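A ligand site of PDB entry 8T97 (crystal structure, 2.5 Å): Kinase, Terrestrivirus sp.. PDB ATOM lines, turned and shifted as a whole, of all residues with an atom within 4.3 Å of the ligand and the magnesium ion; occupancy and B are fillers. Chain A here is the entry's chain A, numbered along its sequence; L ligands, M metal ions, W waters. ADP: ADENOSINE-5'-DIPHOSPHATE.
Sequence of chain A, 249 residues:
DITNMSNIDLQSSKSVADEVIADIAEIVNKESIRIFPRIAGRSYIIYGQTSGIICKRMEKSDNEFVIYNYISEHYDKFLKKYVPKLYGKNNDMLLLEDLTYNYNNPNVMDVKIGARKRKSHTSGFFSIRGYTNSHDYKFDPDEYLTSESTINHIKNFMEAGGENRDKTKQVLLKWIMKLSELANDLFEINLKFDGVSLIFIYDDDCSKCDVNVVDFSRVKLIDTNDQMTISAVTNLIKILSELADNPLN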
ATOM      1  N   PHE A  36      28.154  -2.940  -2.965  1.00  0.00           N
ATOM      2  CA  PHE A  36      28.012  -1.935  -1.874  1.00  0.00           C
ATOM      3  C   PHE A  36      28.147  -2.651  -0.521  1.00  0.00           C
ATOM      4  O   PHE A  36      27.486  -3.666  -0.300  1.00  0.00           O
ATOM      5  CB  PHE A  36      26.695  -1.153  -1.963  1.00  0.00           C
ATOM      6  CG  PHE A  36      26.630   0.024  -1.015  1.00  0.00           C
ATOM      7  CD1 PHE A  36      27.315   1.197  -1.301  1.00  0.00           C
ATOM      8  CD2 PHE A  36      25.962  -0.075   0.196  1.00  0.00           C
ATOM      9  CE1 PHE A  36      27.297   2.269  -0.401  1.00  0.00           C
ATOM     10  CE2 PHE A  36      25.940   0.987   1.087  1.00  0.00           C
ATOM     11  CZ  PHE A  36      26.607   2.165   0.781  1.00  0.00           C
ATOM     12  N   ARG A  38      26.869  -3.309   2.377  1.00  0.00           N
ATOM     13  CA  ARG A  38      25.624  -3.364   3.191  1.00  0.00           C
ATOM     14  C   ARG A  38      25.993  -3.654   4.646  1.00  0.00           C
ATOM     15  O   ARG A  38      27.067  -4.214   4.922  1.00  0.00           O
ATOM     16  CB  ARG A  38      24.671  -4.448   2.659  1.00  0.00           C
ATOM     17  CG  ARG A  38      24.001  -4.078   1.338  1.00  0.00           C
ATOM     18  CD  ARG A  38      24.096  -5.187   0.316  1.00  0.00           C
ATOM     19  NE  ARG A  38      23.218  -6.298   0.669  1.00  0.00           N
ATOM     20  CZ  ARG A  38      23.466  -7.580   0.436  1.00  0.00           C
ATOM     21  NH1 ARG A  38      24.585  -7.976  -0.152  1.00  0.00           N
ATOM     22  NH2 ARG A  38      22.579  -8.487   0.801  1.00  0.00           N
ATOM     23  N   ILE A  39      25.115  -3.258   5.569  1.00  0.00           N
ATOM     24  CA  ILE A  39      25.207  -3.604   7.007  1.00  0.00           C
ATOM     25  C   ILE A  39      24.131  -4.669   7.322  1.00  0.00           C
ATOM     26  O   ILE A  39      24.285  -5.371   8.322  1.00  0.00           O
ATOM     27  CB  ILE A  39      25.127  -2.323   7.872  1.00  0.00           C
ATOM     28  CG1 ILE A  39      26.382  -2.123   8.721  1.00  0.00           C
ATOM     29  CG2 ILE A  39      23.890  -2.300   8.738  1.00  0.00           C
ATOM     30  CD1 ILE A  39      27.682  -2.161   7.959  1.00  0.00           C
ATOM     31  N   ALA A  40      23.117  -4.822   6.469  1.00  0.00           N
ATOM     32  CA  ALA A  40      22.021  -5.811   6.640  1.00  0.00           C
ATOM     33  C   ALA A  40      21.227  -5.977   5.333  1.00  0.00           C
ATOM     34  O   ALA A  40      21.602  -5.339   4.311  1.00  0.00           O
ATOM     35  CB  ALA A  40      21.151  -5.362   7.788  1.00  0.00           C
ATOM     36  N   GLY A  41      20.192  -6.824   5.347  1.00  0.00           N
ATOM     37  CA  GLY A  41      19.315  -7.102   4.195  1.00  0.00           C
ATOM     38  C   GLY A  41      19.880  -8.223   3.339  1.00  0.00           C
ATOM     39  O   GLY A  41      21.032  -8.615   3.583  1.00  0.00           O
ATOM     40  N   ARG A  42      19.091  -8.729   2.373  1.00  0.00           N
ATOM     41  CA  ARG A  42      19.542  -9.731   1.371  1.00  0.00           C
ATOM     42  C   ARG A  42      19.525  -9.119  -0.043  1.00  0.00           C
ATOM     43  O   ARG A  42      20.011  -9.810  -0.985  1.00  0.00           O
ATOM     44  CB  ARG A  42      18.672 -10.989   1.432  1.00  0.00           C
ATOM     45  CG  ARG A  42      19.444 -12.288   1.205  1.00  0.00           C
ATOM     46  CD  ARG A  42      18.586 -13.443   0.677  1.00  0.00           C
ATOM     47  NE  ARG A  42      18.661 -14.629   1.525  1.00  0.00           N
ATOM     48  CZ  ARG A  42      17.827 -15.676   1.450  1.00  0.00           C
ATOM     49  NH1 ARG A  42      16.845 -15.699   0.574  1.00  0.00           N
ATOM     50  NH2 ARG A  42      17.992 -16.705   2.270  1.00  0.00           N
ATOM     51  N   SER A  43      19.032  -7.889  -0.175  1.00  0.00           N
ATOM     52  CA  SER A  43      18.926  -7.096  -1.439  1.00  0.00           C
ATOM     53  C   SER A  43      20.256  -7.041  -2.202  1.00  0.00           C
ATOM     54  O   SER A  43      21.324  -6.830  -1.587  1.00  0.00           O
ATOM     55  CB  SER A  43      18.420  -5.704  -1.177  1.00  0.00           C
ATOM     56  OG  SER A  43      17.029  -5.737  -0.913  1.00  0.00           O
ATOM     57  N   ILE A  45      22.512  -4.815  -3.895  1.00  0.00           N
ATOM     58  CA  ILE A  45      22.873  -3.365  -3.843  1.00  0.00           C
ATOM     59  C   ILE A  45      24.325  -3.218  -4.299  1.00  0.00           C
ATOM     60  O   ILE A  45      25.225  -3.806  -3.656  1.00  0.00           O
ATOM     61  CB  ILE A  45      22.665  -2.711  -2.457  1.00  0.00           C
ATOM     62  CG1 ILE A  45      21.264  -2.989  -1.890  1.00  0.00           C
ATOM     63  CG2 ILE A  45      22.958  -1.213  -2.534  1.00  0.00           C
ATOM     64  CD1 ILE A  45      20.998  -2.360  -0.537  1.00  0.00           C
ATOM     65  N   ILE A  54      23.727   4.564  -5.255  1.00  0.00           N
ATOM     66  CA  ILE A  54      23.706   3.091  -5.110  1.00  0.00           C
ATOM     67  C   ILE A  54      22.500   2.594  -5.881  1.00  0.00           C
ATOM     68  O   ILE A  54      21.507   3.345  -5.986  1.00  0.00           O
ATOM     69  CB  ILE A  54      23.714   2.669  -3.630  1.00  0.00           C
ATOM     70  CG1 ILE A  54      22.538   3.254  -2.859  1.00  0.00           C
ATOM     71  CG2 ILE A  54      25.034   3.042  -2.988  1.00  0.00           C
ATOM     72  CD1 ILE A  54      22.301   2.595  -1.506  1.00  0.00           C
ATOM     73  N   LYS A  56      19.797  -0.352  -6.009  1.00  0.00           N
ATOM     74  CA  LYS A  56      19.113  -1.402  -5.220  1.00  0.00           C
ATOM     75  C   LYS A  56      18.145  -2.097  -6.158  1.00  0.00           C
ATOM     76  O   LYS A  56      17.341  -1.397  -6.788  1.00  0.00           O
ATOM     77  CB  LYS A  56      18.396  -0.804  -4.003  1.00  0.00           C
ATOM     78  CG  LYS A  56      17.402  -1.752  -3.359  1.00  0.00           C
ATOM     79  CD  LYS A  56      16.808  -1.296  -2.066  1.00  0.00           C
ATOM     80  CE  LYS A  56      15.915  -2.361  -1.481  1.00  0.00           C
ATOM     81  NZ  LYS A  56      15.151  -1.850  -0.322  1.00  0.00           N
ATOM     82  N   PRO A  84      16.359   9.044   1.827  1.00  0.00           N
ATOM     83  CA  PRO A  84      17.319   9.248   0.763  1.00  0.00           C
ATOM     84  C   PRO A  84      16.543   9.546  -0.524  1.00  0.00           C
ATOM     85  O   PRO A  84      15.499   8.966  -0.782  1.00  0.00           O
ATOM     86  CB  PRO A  84      18.016   7.902   0.654  1.00  0.00           C
ATOM     87  CG  PRO A  84      16.973   6.953   1.207  1.00  0.00           C
ATOM     88  CD  PRO A  84      16.428   7.706   2.394  1.00  0.00           C
ATOM     89  N   LEU A  96      19.479   5.502  -5.889  1.00  0.00           N
ATOM     90  CA  LEU A  96      19.249   6.123  -4.569  1.00  0.00           C
ATOM     91  C   LEU A  96      20.495   6.903  -4.174  1.00  0.00           C
ATOM     92  O   LEU A  96      21.600   6.451  -4.511  1.00  0.00           O
ATOM     93  CB  LEU A  96      18.976   5.042  -3.513  1.00  0.00           C
ATOM     94  CG  LEU A  96      17.663   4.297  -3.670  1.00  0.00           C
ATOM     95  CD1 LEU A  96      17.593   3.115  -2.699  1.00  0.00           C
ATOM     96  CD2 LEU A  96      16.477   5.223  -3.473  1.00  0.00           C
ATOM     97  N   GLU A  97      20.293   8.001  -3.472  1.00  0.00           N
ATOM     98  CA  GLU A  97      21.368   8.749  -2.790  1.00  0.00           C
ATOM     99  C   GLU A  97      22.101   7.761  -1.892  1.00  0.00           C
ATOM    100  O   GLU A  97      21.442   7.035  -1.172  1.00  0.00           O
ATOM    101  CB  GLU A  97      20.771   9.931  -2.052  1.00  0.00           C
ATOM    102  CG  GLU A  97      21.726  10.611  -1.088  1.00  0.00           C
ATOM    103  CD  GLU A  97      21.025  11.588  -0.154  1.00  0.00           C
ATOM    104  OE1 GLU A  97      19.781  11.640  -0.172  1.00  0.00           O
ATOM    105  OE2 GLU A  97      21.744  12.240   0.634  1.00  0.00           O
ATOM    106  N   ASP A  98      23.421   7.703  -2.034  1.00  0.00           N
ATOM    107  CA  ASP A  98      24.332   6.968  -1.136  1.00  0.00           C
ATOM    108  C   ASP A  98      24.452   7.779   0.155  1.00  0.00           C
ATOM    109  O   ASP A  98      25.117   8.805   0.151  1.00  0.00           O
ATOM    110  CB  ASP A  98      25.715   6.777  -1.753  1.00  0.00           C
ATOM    111  CG  ASP A  98      26.580   5.905  -0.851  1.00  0.00           C
ATOM    112  OD1 ASP A  98      26.130   5.662   0.252  1.00  0.00           O
ATOM    113  OD2 ASP A  98      27.675   5.523  -1.246  1.00  0.00           O
ATOM    114  N   LEU A  99      23.855   7.282   1.231  1.00  0.00           N
ATOM    115  CA  LEU A  99      23.847   8.004   2.541  1.00  0.00           C
ATOM    116  C   LEU A  99      25.258   8.024   3.136  1.00  0.00           C
ATOM    117  O   LEU A  99      25.473   8.862   3.995  1.00  0.00           O
ATOM    118  CB  LEU A  99      22.833   7.326   3.461  1.00  0.00           C
ATOM    119  CG  LEU A  99      21.387   7.464   2.984  1.00  0.00           C
ATOM    120  CD1 LEU A  99      20.462   6.608   3.820  1.00  0.00           C
ATOM    121  CD2 LEU A  99      20.934   8.920   3.000  1.00  0.00           C
ATOM    122  N   THR A 100      26.188   7.199   2.663  1.00  0.00           N
ATOM    123  CA  THR A 100      27.578   7.167   3.214  1.00  0.00           C
ATOM    124  C   THR A 100      28.502   8.074   2.421  1.00  0.00           C
ATOM    125  O   THR A 100      29.615   8.281   2.902  1.00  0.00           O
ATOM    126  CB  THR A 100      28.138   5.739   3.285  1.00  0.00           C
ATOM    127  OG1 THR A 100      28.232   5.193   1.976  1.00  0.00           O
ATOM    128  CG2 THR A 100      27.286   4.811   4.126  1.00  0.00           C
ATOM    129  N   VAL A 108      27.849   2.850  10.255  1.00  0.00           N
ATOM    130  CA  VAL A 108      26.417   2.685   9.905  1.00  0.00           C
ATOM    131  C   VAL A 108      25.775   1.728  10.899  1.00  0.00           C
ATOM    132  O   VAL A 108      26.385   0.682  11.169  1.00  0.00           O
ATOM    133  CB  VAL A 108      26.274   2.199   8.454  1.00  0.00           C
ATOM    134  CG1 VAL A 108      24.808   2.165   8.043  1.00  0.00           C
ATOM    135  CG2 VAL A 108      27.091   3.075   7.506  1.00  0.00           C
ATOM    136  N   ASP A 110      21.840  -0.230  11.137  1.00  0.00           N
ATOM    137  CA  ASP A 110      20.469  -0.490  10.616  1.00  0.00           C
ATOM    138  C   ASP A 110      19.620  -0.930  11.808  1.00  0.00           C
ATOM    139  O   ASP A 110      19.999  -1.904  12.490  1.00  0.00           O
ATOM    140  CB  ASP A 110      20.469  -1.503   9.455  1.00  0.00           C
ATOM    141  CG  ASP A 110      19.100  -1.892   8.879  1.00  0.00           C
ATOM    142  OD1 ASP A 110      18.095  -1.799   9.605  1.00  0.00           O
ATOM    143  OD2 ASP A 110      19.040  -2.323   7.694  1.00  0.00           O
ATOM    144  N   GLY A 195       8.422  -3.088   7.812  1.00  0.00           N
ATOM    145  CA  GLY A 195       9.733  -3.491   7.267  1.00  0.00           C
ATOM    146  C   GLY A 195      10.745  -2.376   7.228  1.00  0.00           C
ATOM    147  O   GLY A 195      11.901  -2.697   6.986  1.00  0.00           O
ATOM    148  N   SER A 197      13.531   0.575   8.034  1.00  0.00           N
ATOM    149  CA  SER A 197      14.661   0.743   8.962  1.00  0.00           C
ATOM    150  C   SER A 197      15.040   2.222   9.064  1.00  0.00           C
ATOM    151  O   SER A 197      14.705   2.988   8.157  1.00  0.00           O
ATOM    152  CB  SER A 197      15.863  -0.039   8.534  1.00  0.00           C
ATOM    153  OG  SER A 197      15.670  -1.434   8.694  1.00  0.00           O
ATOM    154  N   ILE A 199      18.612   4.141   9.227  1.00  0.00           N
ATOM    155  CA  ILE A 199      20.068   4.067   9.004  1.00  0.00           C
ATOM    156  C   ILE A 199      20.684   5.203   9.779  1.00  0.00           C
ATOM    157  O   ILE A 199      20.551   6.361   9.323  1.00  0.00           O
ATOM    158  CB  ILE A 199      20.397   4.139   7.515  1.00  0.00           C
ATOM    159  CG1 ILE A 199      19.610   3.086   6.746  1.00  0.00           C
ATOM    160  CG2 ILE A 199      21.894   3.999   7.315  1.00  0.00           C
ATOM    161  CD1 ILE A 199      19.769   1.696   7.308  1.00  0.00           C
ATOM    162  N   VAL A 214      14.591   4.167   5.527  1.00  0.00           N
ATOM    163  CA  VAL A 214      14.788   3.427   4.251  1.00  0.00           C
ATOM    164  C   VAL A 214      13.895   2.188   4.147  1.00  0.00           C
ATOM    165  O   VAL A 214      13.382   1.715   5.177  1.00  0.00           O
ATOM    166  CB  VAL A 214      16.267   3.060   4.045  1.00  0.00           C
ATOM    167  CG1 VAL A 214      17.124   4.306   4.076  1.00  0.00           C
ATOM    168  CG2 VAL A 214      16.740   2.017   5.045  1.00  0.00           C
ATOM    169  N   ASP A 215      13.732   1.707   2.921  1.00  0.00           N
ATOM    170  CA  ASP A 215      13.213   0.358   2.566  1.00  0.00           C
ATOM    171  C   ASP A 215      11.701   0.374   2.690  1.00  0.00           C
ATOM    172  O   ASP A 215      11.192  -0.024   3.756  1.00  0.00           O
ATOM    173  CB  ASP A 215      13.809  -0.744   3.438  1.00  0.00           C
ATOM    174  CG  ASP A 215      13.417  -2.130   2.985  1.00  0.00           C
ATOM    175  OD1 ASP A 215      12.612  -2.246   2.030  1.00  0.00           O
ATOM    176  OD2 ASP A 215      13.912  -3.088   3.601  1.00  0.00           O
HETATM  177  PB  ADP L   1      16.550  -4.719   2.244  1.00  0.00           P
HETATM  178  O1B ADP L   1      16.280  -4.853   3.733  1.00  0.00           O
HETATM  179  O2B ADP L   1      17.365  -5.865   1.728  1.00  0.00           O
HETATM  180  O3B ADP L   1      15.259  -4.491   1.451  1.00  0.00           O
HETATM  181  PA  ADP L   1      17.529  -1.948   2.834  1.00  0.00           P
HETATM  182  O1A ADP L   1      17.071  -2.044   4.266  1.00  0.00           O
HETATM  183  O2A ADP L   1      16.850  -0.944   1.961  1.00  0.00           O
HETATM  184  O3A ADP L   1      17.477  -3.373   2.072  1.00  0.00           O
HETATM  185  O5' ADP L   1      19.107  -1.684   2.850  1.00  0.00           O
HETATM  186  C5' ADP L   1      20.029  -2.696   3.298  1.00  0.00           C
HETATM  187  C4' ADP L   1      21.303  -2.046   3.767  1.00  0.00           C
HETATM  188  O4' ADP L   1      21.849  -1.199   2.721  1.00  0.00           O
HETATM  189  C3' ADP L   1      21.211  -1.139   4.998  1.00  0.00           C
HETATM  190  O3' ADP L   1      21.371  -1.917   6.182  1.00  0.00           O
HETATM  191  C2' ADP L   1      22.360  -0.155   4.770  1.00  0.00           C
HETATM  192  O2' ADP L   1      23.617  -0.659   5.181  1.00  0.00           O
HETATM  193  C1' ADP L   1      22.357   0.012   3.248  1.00  0.00           C
HETATM  194  N9  ADP L   1      21.581   1.126   2.674  1.00  0.00           N
HETATM  195  C8  ADP L   1      20.276   1.109   2.198  1.00  0.00           C
HETATM  196  N7  ADP L   1      19.898   2.238   1.630  1.00  0.00           N
HETATM  197  C5  ADP L   1      21.041   3.031   1.661  1.00  0.00           C
HETATM  198  C6  ADP L   1      21.313   4.329   1.173  1.00  0.00           C
HETATM  199  N6  ADP L   1      20.455   5.093   0.493  1.00  0.00           N
HETATM  200  N1  ADP L   1      22.574   4.789   1.329  1.00  0.00           N
HETATM  201  C2  ADP L   1      23.473   4.017   1.963  1.00  0.00           C
HETATM  202  N3  ADP L   1      23.330   2.800   2.477  1.00  0.00           N
HETATM  203  C4  ADP L   1      22.086   2.348   2.289  1.00  0.00           C
HETATM  204 MG    MG M   1      15.506  -3.356   5.110  1.00  0.00          MG
HETATM  205  O   HOH W   1      15.257  -7.829   2.947  1.00  0.00           O
HETATM  206  O   HOH W   2      17.066   1.257   0.469  1.00  0.00           O
HETATM  207  O   HOH W   3      14.667  -2.056   6.584  1.00  0.00           O
HETATM  208  O   HOH W   4      14.221  -5.148   4.788  1.00  0.00           O
HETATM  209  O   HOH W   5      17.403  -3.835   6.504  1.00  0.00           O
HETATM  210  O   HOH W   6      24.872   1.616   4.462  1.00  0.00           O
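The magnesium ion is bound by water W3 (2.1 Å), O1B of the ligand (2.2 Å), O1A of the ligand (2.2 Å), OD2 of Asp 215 (2.2 Å), water W4 (2.2 Å) and water W5 (2.4 Å). The magnesium ion has six donor atoms within binding distance.
Merely in contact with the ligand: Ile 54 (3.3 Å), Gly 41 (3.4 Å), Phe 36 (3.5 Å), Ile 45 (3.6 Å), Asp 98 (3.6 Å), Pro 84 (3.7 Å), Arg 38 (3.9 Å) and Ile 199 (3.9 Å). Hydrophobic or aromatic side chains that line the ligand: Phe 36, Ile 39, Ala 40, Ile 45, Ile 54, Pro 84, Leu 99 and Ile 199. Within 4 Å of the ligand: Phe 36, Arg 38, Ile 39, Ala 40, Gly 41, Arg 42, Ser 43, Ile 45, Ile 54, Lys 56, Pro 84, Glu 97, Asp 98, Leu 99, Asp 110, Ile 199 and Asp 215. The nearest printed residue that does not touch the ligand is Val 214 (4.1 Å).
OD1 of Asp 215 lies within salt-bridge range of NZ of Lys 56. NE of Arg 38 sits at hydrogen-bond distance from O of Ser 43, 3.0 Å away. OD1 of Asp 110 lies within hydrogen-bond range of OG of Ser 197 (2.6 Å). The backbone NH of Ile 54 is in hydrogen-bond range of the backbone carbonyl oxygen of Leu 96, at 2.9 Å. O of Gly 41 is in hydrogen-bond range of NH2 of Arg 38, at 3.2 Å. The guanidinium group (NH2) of Arg 38 lies close to the backbone carbonyl oxygen (O) of Arg 42. The backbone carbonyl oxygen of Ile 45 sits at hydrogen-bond distance from the backbone NH of Phe 36. The side-chain carboxylate of Asp 98 sits at hydrogen-bond distance from the side-chain hydroxyl of Thr 100 (2.8 Å).
The backbone NH (N) of Ser 43 lies close to an oxygen (O2B) of the ligand (3.2 Å). An oxygen (O2B) of the ligand lies within hydrogen-bond range of the side-chain hydroxyl of Ser 43, at 2.7 Å. The backbone carbonyl oxygen (O) of Glu 97 lies within hydrogen-bond range of a nitrogen (N6) of the ligand (2.7 Å). N1 of the ligand lies within hydrogen-bond range of N of Leu 99. OD2 of Asp 110 is in hydrogen-bond range of O3' of the ligand, 2.8 Å away. O2A of the ligand lies within salt-bridge range of NZ of Lys 56, at 3.0 Å. An oxygen (O2') of the ligand sits at hydrogen-bond distance from the backbone NH (N) of Ile 39. The backbone NH of Ala 40 lies within hydrogen-bond range of an oxygen (O3') of the ligand (3.4 Å). An oxygen (O2B) of the ligand sits at hydrogen-bond distance from the backbone NH of Arg 42.
Water W3 bridges OG of Ser 197 and O of Gly 195.
Of the 23 residues printed, 1 comes within 4 Å of the magnesium ion. The nearest printed residue that does not touch the magnesium ion is Ser 197 (4.1 Å).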
